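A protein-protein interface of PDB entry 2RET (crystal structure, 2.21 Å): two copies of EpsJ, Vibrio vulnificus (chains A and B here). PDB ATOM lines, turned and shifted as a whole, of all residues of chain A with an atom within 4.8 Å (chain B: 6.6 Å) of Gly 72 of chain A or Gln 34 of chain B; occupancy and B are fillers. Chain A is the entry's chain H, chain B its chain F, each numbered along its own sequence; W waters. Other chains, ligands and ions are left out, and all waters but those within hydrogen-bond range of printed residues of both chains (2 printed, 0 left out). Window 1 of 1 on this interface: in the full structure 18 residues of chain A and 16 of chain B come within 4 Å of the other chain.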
ATOM      1  N   ARG A  70     -17.998  23.186 -11.466  1.00  0.00           N
ATOM      2  CA  ARG A  70     -18.649  21.905 -11.476  1.00  0.00           C
ATOM      3  C   ARG A  70     -20.067  21.915 -12.051  1.00  0.00           C
ATOM      4  O   ARG A  70     -20.772  22.934 -12.028  1.00  0.00           O
ATOM      5  CB  ARG A  70     -18.681  21.296 -10.083  1.00  0.00           C
ATOM      6  CG  ARG A  70     -19.380  22.035  -9.010  1.00  0.00           C
ATOM      7  CD  ARG A  70     -19.905  21.011  -7.962  1.00  0.00           C
ATOM      8  NE  ARG A  70     -21.150  20.397  -8.376  1.00  0.00           N
ATOM      9  CZ  ARG A  70     -21.945  19.635  -7.616  1.00  0.00           C
ATOM     10  NH1 ARG A  70     -21.631  19.322  -6.370  1.00  0.00           N
ATOM     11  NH2 ARG A  70     -23.074  19.148  -8.122  1.00  0.00           N
ATOM     12  N   LEU A  71     -20.456  20.752 -12.571  1.00  0.00           N
ATOM     13  CA  LEU A  71     -21.821  20.496 -13.015  1.00  0.00           C
ATOM     14  C   LEU A  71     -22.746  20.557 -11.819  1.00  0.00           C
ATOM     15  O   LEU A  71     -22.614  19.764 -10.923  1.00  0.00           O
ATOM     16  CB  LEU A  71     -21.905  19.127 -13.680  1.00  0.00           C
ATOM     17  CG  LEU A  71     -20.851  18.939 -14.793  1.00  0.00           C
ATOM     18  CD1 LEU A  71     -20.716  17.432 -15.268  1.00  0.00           C
ATOM     19  CD2 LEU A  71     -21.100  19.913 -15.986  1.00  0.00           C
ATOM     20  N   GLY A  72     -23.660  21.519 -11.799  1.00  0.00           N
ATOM     21  CA  GLY A  72     -24.662  21.672 -10.710  1.00  0.00           C
ATOM     22  C   GLY A  72     -25.926  20.854 -10.954  1.00  0.00           C
ATOM     23  O   GLY A  72     -26.367  20.110 -10.089  1.00  0.00           O
ATOM     24  N   TRP A  73     -26.508  20.963 -12.140  1.00  0.00           N
ATOM     25  CA  TRP A  73     -27.639  20.095 -12.505  1.00  0.00           C
ATOM     26  C   TRP A  73     -27.979  20.221 -13.999  1.00  0.00           C
ATOM     27  O   TRP A  73     -27.514  21.140 -14.658  1.00  0.00           O
ATOM     28  CB  TRP A  73     -28.882  20.399 -11.634  1.00  0.00           C
ATOM     29  CG  TRP A  73     -29.233  21.832 -11.637  1.00  0.00           C
ATOM     30  CD1 TRP A  73     -29.863  22.504 -12.637  1.00  0.00           C
ATOM     31  CD2 TRP A  73     -28.956  22.798 -10.615  1.00  0.00           C
ATOM     32  NE1 TRP A  73     -29.964  23.828 -12.318  1.00  0.00           N
ATOM     33  CE2 TRP A  73     -29.425  24.036 -11.077  1.00  0.00           C
ATOM     34  CE3 TRP A  73     -28.345  22.738  -9.357  1.00  0.00           C
ATOM     35  CZ2 TRP A  73     -29.336  25.199 -10.318  1.00  0.00           C
ATOM     36  CZ3 TRP A  73     -28.233  23.887  -8.621  1.00  0.00           C
ATOM     37  CH2 TRP A  73     -28.726  25.105  -9.096  1.00  0.00           C
ATOM     38  N   HIS A  74     -28.784  19.285 -14.507  1.00  0.00           N
ATOM     39  CA  HIS A  74     -29.351  19.367 -15.845  1.00  0.00           C
ATOM     40  C   HIS A  74     -30.610  20.193 -15.725  1.00  0.00           C
ATOM     41  O   HIS A  74     -31.359  20.035 -14.767  1.00  0.00           O
ATOM     42  CB  HIS A  74     -29.682  17.978 -16.429  1.00  0.00           C
ATOM     43  CG  HIS A  74     -28.475  17.125 -16.676  1.00  0.00           C
ATOM     44  ND1 HIS A  74     -27.834  16.443 -15.662  1.00  0.00           N
ATOM     45  CD2 HIS A  74     -27.764  16.877 -17.804  1.00  0.00           C
ATOM     46  CE1 HIS A  74     -26.790  15.800 -16.153  1.00  0.00           C
ATOM     47  NE2 HIS A  74     -26.726  16.041 -17.454  1.00  0.00           N
ATOM     48  N   GLU A  84     -26.651  23.609 -15.667  1.00  0.00           N
ATOM     49  CA  GLU A  84     -26.141  24.747 -14.903  1.00  0.00           C
ATOM     50  C   GLU A  84     -24.815  24.368 -14.281  1.00  0.00           C
ATOM     51  O   GLU A  84     -24.706  23.343 -13.604  1.00  0.00           O
ATOM     52  CB  GLU A  84     -27.103  25.188 -13.798  1.00  0.00           C
ATOM     53  CG  GLU A  84     -28.334  25.929 -14.246  1.00  0.00           C
ATOM     54  CD  GLU A  84     -28.052  27.066 -15.181  1.00  0.00           C
ATOM     55  OE1 GLU A  84     -27.044  27.751 -14.933  1.00  0.00           O
ATOM     56  OE2 GLU A  84     -28.833  27.274 -16.147  1.00  0.00           O
ATOM     57  N   VAL A  85     -23.823  25.201 -14.529  1.00  0.00           N
ATOM     58  CA  VAL A  85     -22.492  25.055 -14.001  1.00  0.00           C
ATOM     59  C   VAL A  85     -22.368  26.006 -12.808  1.00  0.00           C
ATOM     60  O   VAL A  85     -22.683  27.215 -12.902  1.00  0.00           O
ATOM     61  CB  VAL A  85     -21.436  25.389 -15.051  1.00  0.00           C
ATOM     62  CG1 VAL A  85     -20.030  25.196 -14.489  1.00  0.00           C
ATOM     63  CG2 VAL A  85     -21.637  24.549 -16.280  1.00  0.00           C
ATOM     64  N   THR A  86     -21.934  25.431 -11.682  1.00  0.00           N
ATOM     65  CA  THR A  86     -21.682  26.168 -10.454  1.00  0.00           C
ATOM     66  C   THR A  86     -20.167  26.227 -10.217  1.00  0.00           C
ATOM     67  O   THR A  86     -19.372  25.839 -11.078  1.00  0.00           O
ATOM     68  CB  THR A  86     -22.458  25.515  -9.300  1.00  0.00           C
ATOM     69  OG1 THR A  86     -22.133  24.133  -9.230  1.00  0.00           O
ATOM     70  CG2 THR A  86     -23.998  25.622  -9.544  1.00  0.00           C
ATOM     71  N   MET B  28     -30.941  21.018  -1.262  1.00  0.00           N
ATOM     72  CA  MET B  28     -32.247  20.624  -1.824  1.00  0.00           C
ATOM     73  C   MET B  28     -32.393  20.819  -3.314  1.00  0.00           C
ATOM     74  O   MET B  28     -33.049  19.999  -3.972  1.00  0.00           O
ATOM     75  CB  MET B  28     -33.364  21.391  -1.166  1.00  0.00           C
ATOM     76  CG  MET B  28     -33.565  21.049   0.272  1.00  0.00           C
ATOM     77  SD  MET B  28     -34.808  22.324   1.034  1.00  0.00           S
ATOM     78  CE  MET B  28     -36.327  22.255  -0.254  1.00  0.00           C
ATOM     79  N   ASP B  29     -31.839  21.914  -3.826  1.00  0.00           N
ATOM     80  CA  ASP B  29     -31.759  22.146  -5.272  1.00  0.00           C
ATOM     81  C   ASP B  29     -30.995  21.001  -5.912  1.00  0.00           C
ATOM     82  O   ASP B  29     -31.417  20.484  -6.927  1.00  0.00           O
ATOM     83  CB  ASP B  29     -30.998  23.436  -5.617  1.00  0.00           C
ATOM     84  CG  ASP B  29     -31.891  24.630  -5.922  1.00  0.00           C
ATOM     85  OD1 ASP B  29     -33.070  24.469  -6.245  1.00  0.00           O
ATOM     86  OD2 ASP B  29     -31.392  25.787  -5.881  1.00  0.00           O
ATOM     87  N   SER B  30     -29.856  20.635  -5.328  1.00  0.00           N
ATOM     88  CA  SER B  30     -29.011  19.588  -5.900  1.00  0.00           C
ATOM     89  C   SER B  30     -29.775  18.268  -6.004  1.00  0.00           C
ATOM     90  O   SER B  30     -29.572  17.516  -6.965  1.00  0.00           O
ATOM     91  CB  SER B  30     -27.688  19.401  -5.136  1.00  0.00           C
ATOM     92  OG  SER B  30     -27.816  18.663  -3.898  1.00  0.00           O
ATOM     93  N   ASP B  31     -30.643  17.997  -5.031  1.00  0.00           N
ATOM     94  CA  ASP B  31     -31.427  16.757  -5.031  1.00  0.00           C
ATOM     95  C   ASP B  31     -32.678  16.800  -5.917  1.00  0.00           C
ATOM     96  O   ASP B  31     -32.896  15.905  -6.729  1.00  0.00           O
ATOM     97  CB  ASP B  31     -31.880  16.395  -3.627  1.00  0.00           C
ATOM     98  CG  ASP B  31     -30.751  15.995  -2.728  1.00  0.00           C
ATOM     99  OD1 ASP B  31     -29.712  15.521  -3.207  1.00  0.00           O
ATOM    100  OD2 ASP B  31     -30.932  16.147  -1.500  1.00  0.00           O
ATOM    101  N   PHE B  32     -33.506  17.811  -5.725  1.00  0.00           N
ATOM    102  CA  PHE B  32     -34.868  17.793  -6.273  1.00  0.00           C
ATOM    103  C   PHE B  32     -34.865  18.171  -7.769  1.00  0.00           C
ATOM    104  O   PHE B  32     -35.800  17.843  -8.511  1.00  0.00           O
ATOM    105  CB  PHE B  32     -35.816  18.723  -5.483  1.00  0.00           C
ATOM    106  CG  PHE B  32     -36.300  18.149  -4.170  1.00  0.00           C
ATOM    107  CD1 PHE B  32     -37.402  17.289  -4.137  1.00  0.00           C
ATOM    108  CD2 PHE B  32     -35.702  18.502  -2.978  1.00  0.00           C
ATOM    109  CE1 PHE B  32     -37.846  16.753  -2.933  1.00  0.00           C
ATOM    110  CE2 PHE B  32     -36.134  17.971  -1.779  1.00  0.00           C
ATOM    111  CZ  PHE B  32     -37.207  17.086  -1.751  1.00  0.00           C
ATOM    112  N   ARG B  33     -33.826  18.883  -8.200  1.00  0.00           N
ATOM    113  CA  ARG B  33     -33.652  19.171  -9.617  1.00  0.00           C
ATOM    114  C   ARG B  33     -33.027  18.002 -10.369  1.00  0.00           C
ATOM    115  O   ARG B  33     -32.952  18.043 -11.597  1.00  0.00           O
ATOM    116  CB  ARG B  33     -32.756  20.379  -9.803  1.00  0.00           C
ATOM    117  CG  ARG B  33     -33.368  21.694  -9.450  1.00  0.00           C
ATOM    118  CD  ARG B  33     -32.316  22.703  -9.744  1.00  0.00           C
ATOM    119  NE  ARG B  33     -32.612  24.056  -9.329  1.00  0.00           N
ATOM    120  CZ  ARG B  33     -33.080  25.017 -10.124  1.00  0.00           C
ATOM    121  NH1 ARG B  33     -33.309  24.814 -11.410  1.00  0.00           N
ATOM    122  NH2 ARG B  33     -33.253  26.232  -9.627  1.00  0.00           N
ATOM    123  N   GLN B  34     -32.548  16.997  -9.644  1.00  0.00           N
ATOM    124  CA  GLN B  34     -31.967  15.820 -10.245  1.00  0.00           C
ATOM    125  C   GLN B  34     -32.684  14.509  -9.930  1.00  0.00           C
ATOM    126  O   GLN B  34     -32.058  13.472  -9.822  1.00  0.00           O
ATOM    127  CB  GLN B  34     -30.497  15.742  -9.848  1.00  0.00           C
ATOM    128  CG  GLN B  34     -29.772  17.037 -10.223  1.00  0.00           C
ATOM    129  CD  GLN B  34     -28.386  16.810 -10.621  1.00  0.00           C
ATOM    130  OE1 GLN B  34     -28.081  16.690 -11.816  1.00  0.00           O
ATOM    131  NE2 GLN B  34     -27.508  16.751  -9.643  1.00  0.00           N
ATOM    132  N   ILE B  35     -34.001  14.549  -9.876  1.00  0.00           N
ATOM    133  CA  ILE B  35     -34.807  13.334  -9.666  1.00  0.00           C
ATOM    134  C   ILE B  35     -34.642  12.428 -10.876  1.00  0.00           C
ATOM    135  O   ILE B  35     -34.736  12.894 -11.999  1.00  0.00           O
ATOM    136  CB  ILE B  35     -36.310  13.688  -9.412  1.00  0.00           C
ATOM    137  CG1 ILE B  35     -36.443  14.499  -8.109  1.00  0.00           C
ATOM    138  CG2 ILE B  35     -37.194  12.420  -9.328  1.00  0.00           C
ATOM    139  CD1 ILE B  35     -37.888  15.033  -7.809  1.00  0.00           C
ATOM    140  N   ALA B  36     -34.382  11.144 -10.626  1.00  0.00           N
ATOM    141  CA  ALA B  36     -34.185  10.138 -11.675  1.00  0.00           C
ATOM    142  C   ALA B  36     -35.458   9.329 -11.872  1.00  0.00           C
ATOM    143  O   ALA B  36     -36.136   8.941 -10.905  1.00  0.00           O
ATOM    144  CB  ALA B  36     -33.027   9.212 -11.338  1.00  0.00           C
ATOM    145  N   PHE B  68     -36.690   9.407  -3.072  1.00  0.00           N
ATOM    146  CA  PHE B  68     -36.602   9.223  -4.546  1.00  0.00           C
ATOM    147  C   PHE B  68     -35.152   8.911  -5.010  1.00  0.00           C
ATOM    148  O   PHE B  68     -34.189   9.183  -4.309  1.00  0.00           O
ATOM    149  CB  PHE B  68     -37.139  10.458  -5.274  1.00  0.00           C
ATOM    150  CG  PHE B  68     -36.512  11.756  -4.813  1.00  0.00           C
ATOM    151  CD1 PHE B  68     -37.045  12.458  -3.740  1.00  0.00           C
ATOM    152  CD2 PHE B  68     -35.361  12.273  -5.441  1.00  0.00           C
ATOM    153  CE1 PHE B  68     -36.450  13.652  -3.290  1.00  0.00           C
ATOM    154  CE2 PHE B  68     -34.785  13.471  -5.022  1.00  0.00           C
ATOM    155  CZ  PHE B  68     -35.320  14.159  -3.940  1.00  0.00           C
ATOM    156  N   ALA B  69     -35.028   8.291  -6.177  1.00  0.00           N
ATOM    157  CA  ALA B  69     -33.749   8.073  -6.847  1.00  0.00           C
ATOM    158  C   ALA B  69     -33.357   9.412  -7.441  1.00  0.00           C
ATOM    159  O   ALA B  69     -34.214  10.185  -7.786  1.00  0.00           O
ATOM    160  CB  ALA B  69     -33.870   7.015  -7.936  1.00  0.00           C
ATOM    161  N   ARG B  70     -32.064   9.712  -7.488  1.00  0.00           N
ATOM    162  CA  ARG B  70     -31.593  10.908  -8.163  1.00  0.00           C
ATOM    163  C   ARG B  70     -30.277  10.640  -8.930  1.00  0.00           C
ATOM    164  O   ARG B  70     -29.564   9.668  -8.614  1.00  0.00           O
ATOM    165  CB  ARG B  70     -31.427  12.047  -7.151  1.00  0.00           C
ATOM    166  CG  ARG B  70     -30.392  11.829  -6.061  1.00  0.00           C
ATOM    167  CD  ARG B  70     -29.741  13.165  -5.635  1.00  0.00           C
ATOM    168  NE  ARG B  70     -28.729  13.623  -6.567  1.00  0.00           N
ATOM    169  CZ  ARG B  70     -27.810  14.577  -6.335  1.00  0.00           C
ATOM    170  NH1 ARG B  70     -27.745  15.234  -5.191  1.00  0.00           N
ATOM    171  NH2 ARG B  70     -26.939  14.902  -7.278  1.00  0.00           N
ATOM    172  N   LEU B  71     -29.963  11.471  -9.930  1.00  0.00           N
ATOM    173  CA  LEU B  71     -28.658  11.391 -10.586  1.00  0.00           C
ATOM    174  C   LEU B  71     -27.594  11.880  -9.636  1.00  0.00           C
ATOM    175  O   LEU B  71     -27.622  13.034  -9.205  1.00  0.00           O
ATOM    176  CB  LEU B  71     -28.559  12.172 -11.919  1.00  0.00           C
ATOM    177  CG  LEU B  71     -27.195  11.876 -12.625  1.00  0.00           C
ATOM    178  CD1 LEU B  71     -27.184  10.486 -13.324  1.00  0.00           C
ATOM    179  CD2 LEU B  71     -26.686  12.976 -13.617  1.00  0.00           C
ATOM    180  N   GLY B  72     -26.638  11.004  -9.335  1.00  0.00           N
ATOM    181  CA  GLY B  72     -25.538  11.315  -8.470  1.00  0.00           C
ATOM    182  C   GLY B  72     -24.454  12.004  -9.235  1.00  0.00           C
ATOM    183  O   GLY B  72     -24.055  13.098  -8.876  1.00  0.00           O
ATOM    184  N   TRP B  73     -23.979  11.359 -10.298  1.00  0.00           N
ATOM    185  CA  TRP B  73     -22.940  11.932 -11.176  1.00  0.00           C
ATOM    186  C   TRP B  73     -22.810  11.164 -12.502  1.00  0.00           C
ATOM    187  O   TRP B  73     -23.220  10.036 -12.599  1.00  0.00           O
ATOM    188  CB  TRP B  73     -21.573  11.963 -10.466  1.00  0.00           C
ATOM    189  CG  TRP B  73     -21.169  10.644  -9.944  1.00  0.00           C
ATOM    190  CD1 TRP B  73     -20.612   9.606 -10.656  1.00  0.00           C
ATOM    191  CD2 TRP B  73     -21.308  10.177  -8.604  1.00  0.00           C
ATOM    192  NE1 TRP B  73     -20.398   8.540  -9.842  1.00  0.00           N
ATOM    193  CE2 TRP B  73     -20.819   8.855  -8.574  1.00  0.00           C
ATOM    194  CE3 TRP B  73     -21.787  10.753  -7.417  1.00  0.00           C
ATOM    195  CZ2 TRP B  73     -20.799   8.098  -7.406  1.00  0.00           C
ATOM    196  CZ3 TRP B  73     -21.768  10.010  -6.273  1.00  0.00           C
ATOM    197  CH2 TRP B  73     -21.285   8.694  -6.268  1.00  0.00           C
ATOM    198  N   LEU B 166     -38.936  21.075 -11.527  1.00  0.00           N
ATOM    199  CA  LEU B 166     -39.408  20.320 -12.682  1.00  0.00           C
ATOM    200  C   LEU B 166     -38.706  18.983 -12.752  1.00  0.00           C
ATOM    201  O   LEU B 166     -37.526  18.863 -12.435  1.00  0.00           O
ATOM    202  CB  LEU B 166     -39.188  21.090 -14.001  1.00  0.00           C
ATOM    203  CG  LEU B 166     -39.926  22.417 -14.214  1.00  0.00           C
ATOM    204  CD1 LEU B 166     -39.861  22.858 -15.668  1.00  0.00           C
ATOM    205  CD2 LEU B 166     -41.364  22.308 -13.786  1.00  0.00           C
ATOM    206  N   PRO B 168     -37.777  15.221 -14.864  1.00  0.00           N
ATOM    207  CA  PRO B 168     -37.524  14.748 -16.219  1.00  0.00           C
ATOM    208  C   PRO B 168     -38.717  14.043 -16.865  1.00  0.00           C
ATOM    209  O   PRO B 168     -39.423  13.281 -16.205  1.00  0.00           O
ATOM    210  CB  PRO B 168     -36.339  13.781 -16.050  1.00  0.00           C
ATOM    211  CG  PRO B 168     -36.389  13.339 -14.630  1.00  0.00           C
ATOM    212  CD  PRO B 168     -37.010  14.463 -13.851  1.00  0.00           C
HETATM  213  O   HOH W   1     -33.672  20.087 -13.265  1.00  0.00           O
HETATM  214  O   HOH W   2     -25.086  17.473 -10.596  1.00  0.00           O
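OD1 of Asp 29 of chain B lies within salt-bridge range of NE of Arg 33 of chain B, at 3.1 Å. O of Ser 30 of chain B lies close to NE2 of Gln 34 of chain B, 3.5 Å away. The guanidinium group of Arg 70 of chain B sits close to the side-chain amide nitrogen of Gln 34 of chain B. The backbone NH (N) of Leu 71 of chain B lies within hydrogen-bond range of the backbone carbonyl oxygen (O) of Gln 34 of chain B (2.9 Å). The backbone NH of Gly 72 of chain A lies within hydrogen-bond range of the backbone carbonyl oxygen of Glu 84 of chain A (2.8 Å). O of Trp 73 of chain A is in hydrogen-bond range of N of Glu 84 of chain A, 2.8 Å away.
Gly 72 of chain A touches Gln 34 of chain B. Trp 73 of chain A touches Arg 33 of chain B (CE2 to CD, 3.5 Å). OE1 of Gln 34 of chain B touches CA of Trp 73 of chain A, at 3.5 Å. Gln 34 of chain B touches His 74 of chain A. Leu 71 of chain B touches His 74 of chain A.
Gly 72 of chain A touches one residue of chain B. Of the printed residues of chain B, Trp 73 of chain A touches Arg 33 and Gln 34. Asp 29 of chain B touches none of the printed residues of chain A. Of the printed residues of chain A, Arg 33 of chain B touches Trp 73. Of chain A, only Gly 72, Trp 73 and His 74 come within 4 Å of Gln 34 of chain B. Gly 72 of chain B touches none of the printed residues of chain A. The nearest residue of chain B that does not touch Gly 72 of chain A is Ser 30 of chain B (5.0 Å). The nearest printed residue of chain A that does not touch Leu 71 of chain B is Gly 72 of chain A (7.2 Å).
Of the 8 printed residues of chain A, 3 touch a printed residue of chain B. Of the 17 printed residues of chain B, 3 touch a printed residue of chain A. Printed residues of chain B that touch a printed residue of chain A: Arg 33, Gln 34 and Leu 71. Hydrophobic or aromatic side chains of chain B that line the printed part of chain A: Leu 71. Along chain B the printed residues that touch a printed residue of chain A span positions 33 to 71. Among the printed residues, 5 pairs touch across the chains.
Positions printed for both chains: 70, 71, 72 and 73. Of the 5 pairs that touch across the chains among the printed residues, none has its exchanged pair printed and touching as well.
Water W2 lies within hydrogen-bond range of the side-chain amide nitrogen of Gln 34 of chain B (2.7 Å), the backbone carbonyl oxygen of Gly 72 of chain A (3.0 Å) and the backbone carbonyl oxygen of Leu 71 of chain A (3.4 Å). Water W1 bridges O of Arg 33 of chain B (2.7 Å) and O of His 74 of chain A (2.8 Å).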
